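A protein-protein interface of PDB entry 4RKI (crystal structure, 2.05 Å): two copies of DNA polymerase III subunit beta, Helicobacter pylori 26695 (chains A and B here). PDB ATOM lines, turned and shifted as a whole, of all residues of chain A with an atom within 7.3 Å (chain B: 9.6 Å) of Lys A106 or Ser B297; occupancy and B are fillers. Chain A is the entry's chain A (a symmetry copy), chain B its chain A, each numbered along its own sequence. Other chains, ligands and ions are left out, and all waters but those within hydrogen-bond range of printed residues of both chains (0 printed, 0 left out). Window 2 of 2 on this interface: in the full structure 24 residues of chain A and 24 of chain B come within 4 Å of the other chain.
Ile A78 touches Ser B273.
Ile A78 touches Leu B274 (CD1 to CD1, 3.9 Å).
O of Ser A104 touches CA of Ala B300, 3.7 Å away.
CD2 of Leu B270 touches CZ of Phe A105, at 3.4 Å.
Phe A105 touches Thr B299 (CA to O, 3.2 Å).
CB of Ala B300 touches CD2 of Phe A105, at 3.5 Å.
Lys A106 touches Glu B298.
Leu B274 touches Leu A107 (CD2 to CD2, 3.9 Å).
Leu A107 touches Glu B298 (CD2 to CG, 3.7 Å).
Pro A108 touches Glu B298 (CD to CG, 3.6 Å).
Of the 15 printed residues of chain A, 6 touch a printed residue of chain B.
Of the 13 printed residues of chain B, 8 touch a printed residue of chain A.
Printed residues of chain B that touch a printed residue of chain A: Leu B270, Ser B273, Leu B274, Ser B297, Glu B298, Thr B299, Ala B300 and Lys B301.
Among the printed residues, 15 pairs touch across the chains.
N of Lys A106 sits at hydrogen-bond distance from O of Thr B299 (2.9 Å).
O of Ser A104 lies within hydrogen-bond range of N of Lys B301 (2.9 Å).
OG of Ser B273 lies within hydrogen-bond range of O of Leu B270 (2.6 Å).
O of Ala B300 lies within hydrogen-bond range of N of Ser B291, 2.8 Å away.
The side-chain hydroxyl (OG) of Ser B294 lies within hydrogen-bond range of the backbone carbonyl oxygen (O) of Glu B298 (2.8 Å).
The backbone NH (N) of Leu A96 is in hydrogen-bond range of the backbone carbonyl oxygen (O) of Leu A107 (2.8 Å).
N of Phe A105 sits at hydrogen-bond distance from O of Ile A98 (2.7 Å).
No position is printed for both chains.
Of the 15 pairs that touch across the chains among the printed residues, none has its exchanged pair printed and touching as well.
Of chain B, only Ser B297, Glu B298 and Thr B299 come within 4 Å of Lys A106.
Of the printed residues of chain A, Ser B297 touches Lys A106 (3.8 Å), Leu A107 (3.9 Å) and Pro A108 (3.4 Å).
Of chain B, only Leu B274, Ser B297 and Glu B298 come within 4 Å of Leu A107.
Of the printed residues of chain B, Ile A78 touches Ser B273 and Leu B274.
Of the printed residues of chain A, Thr B299 touches Phe A105 (3.2 Å) and Lys A106 (2.9 Å).
Of the printed residues of chain A, Lys B301 touches Ser A104.
Printed residues of chain A within 4 Å of Ala B300: Ser A104 and Phe A105.
Lys A99 touches none of the printed residues of chain B.
The nearest residue of chain A that does not touch Ser B297 is Ser A95 (5.3 Å).
The nearest printed residue of chain B that does not touch Pro A108 is His B296 (4.9 Å).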
ATOM      1  N   ILE A  70     -16.437  15.511  25.999  1.00  0.00           N
ATOM      2  CA  ILE A  70     -15.646  16.288  25.050  1.00  0.00           C
ATOM      3  C   ILE A  70     -16.538  16.892  23.977  1.00  0.00           C
ATOM      4  O   ILE A  70     -17.527  16.278  23.569  1.00  0.00           O
ATOM      5  CB  ILE A  70     -14.564  15.401  24.403  1.00  0.00           C
ATOM      6  CG1 ILE A  70     -13.583  16.262  23.616  1.00  0.00           C
ATOM      7  CG2 ILE A  70     -15.203  14.309  23.544  1.00  0.00           C
ATOM      8  CD1 ILE A  70     -12.416  15.493  23.039  1.00  0.00           C
ATOM      9  N   ILE A  78     -10.712  17.471  14.777  1.00  0.00           N
ATOM     10  CA  ILE A  78      -9.337  17.063  15.058  1.00  0.00           C
ATOM     11  C   ILE A  78      -8.992  15.721  14.421  1.00  0.00           C
ATOM     12  O   ILE A  78      -7.998  15.609  13.701  1.00  0.00           O
ATOM     13  CB  ILE A  78      -9.057  17.000  16.565  1.00  0.00           C
ATOM     14  CG1 ILE A  78      -9.027  18.412  17.142  1.00  0.00           C
ATOM     15  CG2 ILE A  78      -7.725  16.309  16.835  1.00  0.00           C
ATOM     16  CD1 ILE A  78      -9.040  18.456  18.654  1.00  0.00           C
ATOM     17  N   LYS A  92      -6.402  14.142  31.690  1.00  0.00           N
ATOM     18  CA  LYS A  92      -5.409  14.701  32.545  1.00  0.00           C
ATOM     19  C   LYS A  92      -6.153  15.225  33.710  1.00  0.00           C
ATOM     20  O   LYS A  92      -6.387  14.487  34.637  1.00  0.00           O
ATOM     21  CB  LYS A  92      -4.562  15.700  31.819  1.00  0.00           C
ATOM     22  CG  LYS A  92      -3.787  15.000  30.729  1.00  0.00           C
ATOM     23  CD  LYS A  92      -2.358  15.447  30.666  1.00  0.00           C
ATOM     24  CE  LYS A  92      -1.567  14.662  29.646  1.00  0.00           C
ATOM     25  NZ  LYS A  92      -1.927  13.252  29.687  1.00  0.00           N
ATOM     26  N   ASP A  94      -9.337  17.978  34.008  1.00  0.00           N
ATOM     27  CA  ASP A  94     -10.594  18.062  33.318  1.00  0.00           C
ATOM     28  C   ASP A  94     -10.303  18.402  31.872  1.00  0.00           C
ATOM     29  O   ASP A  94     -10.895  19.262  31.312  1.00  0.00           O
ATOM     30  CB  ASP A  94     -11.478  19.096  33.952  1.00  0.00           C
ATOM     31  CG  ASP A  94     -10.692  20.121  34.696  1.00  0.00           C
ATOM     32  OD1 ASP A  94     -10.044  20.941  34.028  1.00  0.00           O
ATOM     33  OD2 ASP A  94     -10.718  20.099  35.945  1.00  0.00           O
ATOM     34  N   SER A  95      -9.366  17.679  31.305  1.00  0.00           N
ATOM     35  CA  SER A  95      -8.955  17.887  29.953  1.00  0.00           C
ATOM     36  C   SER A  95      -8.692  16.544  29.315  1.00  0.00           C
ATOM     37  O   SER A  95      -8.208  15.657  29.974  1.00  0.00           O
ATOM     38  CB  SER A  95      -7.708  18.758  29.950  1.00  0.00           C
ATOM     39  OG  SER A  95      -6.997  18.674  28.758  1.00  0.00           O
ATOM     40  N   LEU A  96      -9.051  16.398  28.041  1.00  0.00           N
ATOM     41  CA  LEU A  96      -8.767  15.185  27.263  1.00  0.00           C
ATOM     42  C   LEU A  96      -7.584  15.418  26.338  1.00  0.00           C
ATOM     43  O   LEU A  96      -7.608  16.330  25.506  1.00  0.00           O
ATOM     44  CB  LEU A  96      -9.980  14.723  26.448  1.00  0.00           C
ATOM     45  CG  LEU A  96      -9.770  13.417  25.649  1.00  0.00           C
ATOM     46  CD1 LEU A  96      -9.530  12.225  26.551  1.00  0.00           C
ATOM     47  CD2 LEU A  96     -10.922  13.124  24.694  1.00  0.00           C
ATOM     48  N   ALA A  97      -6.539  14.605  26.493  1.00  0.00           N
ATOM     49  CA  ALA A  97      -5.379  14.686  25.606  1.00  0.00           C
ATOM     50  C   ALA A  97      -5.547  13.680  24.491  1.00  0.00           C
ATOM     51  O   ALA A  97      -5.989  12.547  24.721  1.00  0.00           O
ATOM     52  CB  ALA A  97      -4.085  14.444  26.351  1.00  0.00           C
ATOM     53  N   ILE A  98      -5.211  14.113  23.283  1.00  0.00           N
ATOM     54  CA  ILE A  98      -5.298  13.283  22.094  1.00  0.00           C
ATOM     55  C   ILE A  98      -3.936  13.294  21.417  1.00  0.00           C
ATOM     56  O   ILE A  98      -3.402  14.364  21.117  1.00  0.00           O
ATOM     57  CB  ILE A  98      -6.341  13.832  21.117  1.00  0.00           C
ATOM     58  CG1 ILE A  98      -7.699  13.964  21.820  1.00  0.00           C
ATOM     59  CG2 ILE A  98      -6.428  12.951  19.873  1.00  0.00           C
ATOM     60  CD1 ILE A  98      -8.673  14.874  21.111  1.00  0.00           C
ATOM     61  N   LYS A  99      -3.362  12.117  21.196  1.00  0.00           N
ATOM     62  CA  LYS A  99      -2.037  12.043  20.602  1.00  0.00           C
ATOM     63  C   LYS A  99      -1.989  11.033  19.485  1.00  0.00           C
ATOM     64  O   LYS A  99      -2.628   9.979  19.543  1.00  0.00           O
ATOM     65  CB  LYS A  99      -0.983  11.712  21.650  1.00  0.00           C
ATOM     66  CG  LYS A  99      -0.944  12.717  22.781  1.00  0.00           C
ATOM     67  CD  LYS A  99       0.434  12.816  23.410  1.00  0.00           C
ATOM     68  CE  LYS A  99       0.505  13.956  24.415  1.00  0.00           C
ATOM     69  NZ  LYS A  99       1.893  14.487  24.518  1.00  0.00           N
ATOM     70  N   SER A 104      -0.348  16.338  18.879  1.00  0.00           N
ATOM     71  CA  SER A 104      -1.052  16.247  20.159  1.00  0.00           C
ATOM     72  C   SER A 104      -2.038  17.394  20.369  1.00  0.00           C
ATOM     73  O   SER A 104      -1.831  18.511  19.887  1.00  0.00           O
ATOM     74  CB  SER A 104      -0.065  16.159  21.318  1.00  0.00           C
ATOM     75  OG  SER A 104       0.462  17.421  21.644  1.00  0.00           O
ATOM     76  N   PHE A 105      -3.126  17.096  21.074  1.00  0.00           N
ATOM     77  CA  PHE A 105      -4.213  18.051  21.281  1.00  0.00           C
ATOM     78  C   PHE A 105      -4.752  17.978  22.693  1.00  0.00           C
ATOM     79  O   PHE A 105      -4.672  16.931  23.348  1.00  0.00           O
ATOM     80  CB  PHE A 105      -5.370  17.774  20.322  1.00  0.00           C
ATOM     81  CG  PHE A 105      -4.951  17.587  18.892  1.00  0.00           C
ATOM     82  CD1 PHE A 105      -4.384  16.391  18.476  1.00  0.00           C
ATOM     83  CD2 PHE A 105      -5.141  18.597  17.960  1.00  0.00           C
ATOM     84  CE1 PHE A 105      -3.992  16.211  17.169  1.00  0.00           C
ATOM     85  CE2 PHE A 105      -4.757  18.423  16.644  1.00  0.00           C
ATOM     86  CZ  PHE A 105      -4.181  17.225  16.248  1.00  0.00           C
ATOM     87  N   LYS A 106      -5.320  19.085  23.157  1.00  0.00           N
ATOM     88  CA  LYS A 106      -6.067  19.098  24.415  1.00  0.00           C
ATOM     89  C   LYS A 106      -7.412  19.762  24.193  1.00  0.00           C
ATOM     90  O   LYS A 106      -7.503  20.763  23.480  1.00  0.00           O
ATOM     91  CB  LYS A 106      -5.313  19.842  25.504  1.00  0.00           C
ATOM     92  CG  LYS A 106      -4.069  19.127  25.978  1.00  0.00           C
ATOM     93  CD  LYS A 106      -3.549  19.716  27.278  1.00  0.00           C
ATOM     94  CE  LYS A 106      -3.085  21.155  27.098  1.00  0.00           C
ATOM     95  NZ  LYS A 106      -2.205  21.583  28.220  1.00  0.00           N
ATOM     96  N   LEU A 107      -8.448  19.187  24.794  1.00  0.00           N
ATOM     97  CA  LEU A 107      -9.780  19.781  24.802  1.00  0.00           C
ATOM     98  C   LEU A 107     -10.374  19.668  26.211  1.00  0.00           C
ATOM     99  O   LEU A 107     -10.124  18.697  26.910  1.00  0.00           O
ATOM    100  CB  LEU A 107     -10.686  19.080  23.793  1.00  0.00           C
ATOM    101  CG  LEU A 107     -10.580  19.480  22.312  1.00  0.00           C
ATOM    102  CD1 LEU A 107     -11.441  18.557  21.467  1.00  0.00           C
ATOM    103  CD2 LEU A 107     -10.981  20.933  22.080  1.00  0.00           C
ATOM    104  N   PRO A 108     -11.157  20.671  26.628  1.00  0.00           N
ATOM    105  CA  PRO A 108     -11.710  20.653  27.964  1.00  0.00           C
ATOM    106  C   PRO A 108     -12.862  19.654  28.080  1.00  0.00           C
ATOM    107  O   PRO A 108     -13.636  19.486  27.143  1.00  0.00           O
ATOM    108  CB  PRO A 108     -12.185  22.099  28.163  1.00  0.00           C
ATOM    109  CG  PRO A 108     -12.515  22.577  26.783  1.00  0.00           C
ATOM    110  CD  PRO A 108     -11.604  21.842  25.852  1.00  0.00           C
ATOM    111  N   MET A 109     -12.935  18.960  29.213  1.00  0.00           N
ATOM    112  CA  MET A 109     -14.060  18.099  29.500  1.00  0.00           C
ATOM    113  C   MET A 109     -14.979  18.831  30.451  1.00  0.00           C
ATOM    114  O   MET A 109     -14.548  19.741  31.157  1.00  0.00           O
ATOM    115  CB  MET A 109     -13.595  16.801  30.135  1.00  0.00           C
ATOM    116  CG  MET A 109     -12.416  16.166  29.429  1.00  0.00           C
ATOM    117  SD  MET A 109     -12.273  14.426  29.834  1.00  0.00           S
ATOM    118  CE  MET A 109     -12.101  14.479  31.613  1.00  0.00           C
ATOM    119  N   LEU B 270      -4.255  20.747  10.214  1.00  0.00           N
ATOM    120  CA  LEU B 270      -4.383  20.075  11.496  1.00  0.00           C
ATOM    121  C   LEU B 270      -4.562  21.061  12.653  1.00  0.00           C
ATOM    122  O   LEU B 270      -5.496  20.909  13.447  1.00  0.00           O
ATOM    123  CB  LEU B 270      -3.167  19.173  11.716  1.00  0.00           C
ATOM    124  CG  LEU B 270      -3.059  18.400  13.025  1.00  0.00           C
ATOM    125  CD1 LEU B 270      -2.267  17.127  12.790  1.00  0.00           C
ATOM    126  CD2 LEU B 270      -2.428  19.237  14.132  1.00  0.00           C
ATOM    127  N   SER B 273      -7.837  23.145  13.061  1.00  0.00           N
ATOM    128  CA  SER B 273      -9.023  22.524  13.615  1.00  0.00           C
ATOM    129  C   SER B 273      -9.484  23.289  14.857  1.00  0.00           C
ATOM    130  O   SER B 273     -10.671  23.297  15.159  1.00  0.00           O
ATOM    131  CB  SER B 273      -8.787  21.044  13.922  1.00  0.00           C
ATOM    132  OG  SER B 273      -7.735  20.870  14.846  1.00  0.00           O
ATOM    133  N   LEU B 274      -8.557  23.957  15.545  1.00  0.00           N
ATOM    134  CA  LEU B 274      -8.874  24.694  16.765  1.00  0.00           C
ATOM    135  C   LEU B 274      -8.490  26.173  16.751  1.00  0.00           C
ATOM    136  O   LEU B 274      -8.583  26.836  17.785  1.00  0.00           O
ATOM    137  CB  LEU B 274      -8.176  24.024  17.962  1.00  0.00           C
ATOM    138  CG  LEU B 274      -8.590  22.585  18.292  1.00  0.00           C
ATOM    139  CD1 LEU B 274      -7.780  22.063  19.462  1.00  0.00           C
ATOM    140  CD2 LEU B 274     -10.077  22.524  18.592  1.00  0.00           C
ATOM    141  N   SER B 291      -1.327  25.821  17.534  1.00  0.00           N
ATOM    142  CA  SER B 291      -2.457  26.742  17.519  1.00  0.00           C
ATOM    143  C   SER B 291      -2.117  27.978  18.368  1.00  0.00           C
ATOM    144  O   SER B 291      -1.555  27.867  19.452  1.00  0.00           O
ATOM    145  CB  SER B 291      -3.725  26.061  18.036  1.00  0.00           C
ATOM    146  OG  SER B 291      -3.572  25.605  19.374  1.00  0.00           O
ATOM    147  N   ASP B 293      -4.440  31.043  18.069  1.00  0.00           N
ATOM    148  CA  ASP B 293      -5.705  31.751  18.185  1.00  0.00           C
ATOM    149  C   ASP B 293      -6.742  30.971  19.004  1.00  0.00           C
ATOM    150  O   ASP B 293      -7.857  31.446  19.192  1.00  0.00           O
ATOM    151  CB  ASP B 293      -6.241  31.928  16.754  1.00  0.00           C
ATOM    152  CG  ASP B 293      -7.302  32.985  16.631  1.00  0.00           C
ATOM    153  OD1 ASP B 293      -7.073  34.124  17.082  1.00  0.00           O
ATOM    154  OD2 ASP B 293      -8.359  32.678  16.038  1.00  0.00           O
ATOM    155  N   SER B 294      -6.383  29.778  19.476  1.00  0.00           N
ATOM    156  CA  SER B 294      -7.363  28.854  20.058  1.00  0.00           C
ATOM    157  C   SER B 294      -7.887  29.324  21.405  1.00  0.00           C
ATOM    158  O   SER B 294      -7.194  30.029  22.142  1.00  0.00           O
ATOM    159  CB  SER B 294      -6.773  27.443  20.179  1.00  0.00           C
ATOM    160  OG  SER B 294      -5.540  27.447  20.869  1.00  0.00           O
ATOM    161  N   GLU B 295      -9.120  28.917  21.710  1.00  0.00           N
ATOM    162  CA  GLU B 295      -9.784  29.253  22.971  1.00  0.00           C
ATOM    163  C   GLU B 295      -9.030  28.652  24.143  1.00  0.00           C
ATOM    164  O   GLU B 295      -8.240  27.723  23.974  1.00  0.00           O
ATOM    165  CB  GLU B 295     -11.225  28.730  22.982  1.00  0.00           C
ATOM    166  CG  GLU B 295     -12.160  29.394  21.977  1.00  0.00           C
ATOM    167  CD  GLU B 295     -12.835  30.644  22.516  1.00  0.00           C
ATOM    168  OE1 GLU B 295     -12.316  31.250  23.477  1.00  0.00           O
ATOM    169  OE2 GLU B 295     -13.894  31.021  21.975  1.00  0.00           O
ATOM    170  N   HIS B 296      -9.292  29.187  25.330  1.00  0.00           N
ATOM    171  CA  HIS B 296      -8.618  28.756  26.545  1.00  0.00           C
ATOM    172  C   HIS B 296      -8.807  27.255  26.772  1.00  0.00           C
ATOM    173  O   HIS B 296      -9.917  26.726  26.630  1.00  0.00           O
ATOM    174  CB  HIS B 296      -9.141  29.546  27.749  1.00  0.00           C
ATOM    175  CG  HIS B 296      -8.455  29.207  29.035  1.00  0.00           C
ATOM    176  ND1 HIS B 296      -7.085  29.260  29.183  1.00  0.00           N
ATOM    177  CD2 HIS B 296      -8.949  28.817  30.234  1.00  0.00           C
ATOM    178  CE1 HIS B 296      -6.766  28.913  30.418  1.00  0.00           C
ATOM    179  NE2 HIS B 296      -7.878  28.639  31.075  1.00  0.00           N
ATOM    180  N   SER B 297      -7.708  26.582  27.098  1.00  0.00           N
ATOM    181  CA  SER B 297      -7.681  25.135  27.334  1.00  0.00           C
ATOM    182  C   SER B 297      -8.048  24.284  26.103  1.00  0.00           C
ATOM    183  O   SER B 297      -8.466  23.139  26.245  1.00  0.00           O
ATOM    184  CB  SER B 297      -8.553  24.760  28.540  1.00  0.00           C
ATOM    185  OG  SER B 297      -9.930  24.816  28.222  1.00  0.00           O
ATOM    186  N   GLU B 298      -7.877  24.837  24.902  1.00  0.00           N
ATOM    187  CA  GLU B 298      -7.925  24.048  23.680  1.00  0.00           C
ATOM    188  C   GLU B 298      -6.616  24.253  22.941  1.00  0.00           C
ATOM    189  O   GLU B 298      -6.279  25.381  22.596  1.00  0.00           O
ATOM    190  CB  GLU B 298      -9.083  24.478  22.811  1.00  0.00           C
ATOM    191  CG  GLU B 298     -10.431  24.323  23.483  1.00  0.00           C
ATOM    192  CD  GLU B 298     -11.569  24.648  22.554  1.00  0.00           C
ATOM    193  OE1 GLU B 298     -11.299  24.999  21.391  1.00  0.00           O
ATOM    194  OE2 GLU B 298     -12.731  24.546  22.981  1.00  0.00           O
ATOM    195  N   THR B 299      -5.878  23.169  22.717  1.00  0.00           N
ATOM    196  CA  THR B 299      -4.531  23.230  22.139  1.00  0.00           C
ATOM    197  C   THR B 299      -4.402  22.216  21.008  1.00  0.00           C
ATOM    198  O   THR B 299      -4.957  21.122  21.079  1.00  0.00           O
ATOM    199  CB  THR B 299      -3.455  22.940  23.206  1.00  0.00           C
ATOM    200  OG1 THR B 299      -3.386  24.038  24.119  1.00  0.00           O
ATOM    201  CG2 THR B 299      -2.082  22.740  22.586  1.00  0.00           C
ATOM    202  N   ALA B 300      -3.669  22.601  19.967  1.00  0.00           N
ATOM    203  CA  ALA B 300      -3.356  21.719  18.842  1.00  0.00           C
ATOM    204  C   ALA B 300      -1.904  21.945  18.459  1.00  0.00           C
ATOM    205  O   ALA B 300      -1.498  23.078  18.232  1.00  0.00           O
ATOM    206  CB  ALA B 300      -4.270  22.003  17.663  1.00  0.00           C
ATOM    207  N   LYS B 301      -1.119  20.873  18.428  1.00  0.00           N
ATOM    208  CA  LYS B 301       0.283  20.954  18.064  1.00  0.00           C
ATOM    209  C   LYS B 301       0.678  19.794  17.178  1.00  0.00           C
ATOM    210  O   LYS B 301       0.137  18.685  17.288  1.00  0.00           O
ATOM    211  CB  LYS B 301       1.182  20.903  19.290  1.00  0.00           C
ATOM    212  CG  LYS B 301       0.916  21.952  20.351  1.00  0.00           C
ATOM    213  CD  LYS B 301       1.652  21.618  21.641  1.00  0.00           C
ATOM    214  CE  LYS B 301       3.101  21.195  21.409  1.00  0.00           C
ATOM    215  NZ  LYS B 301       3.807  20.921  22.693  1.00  0.00           N
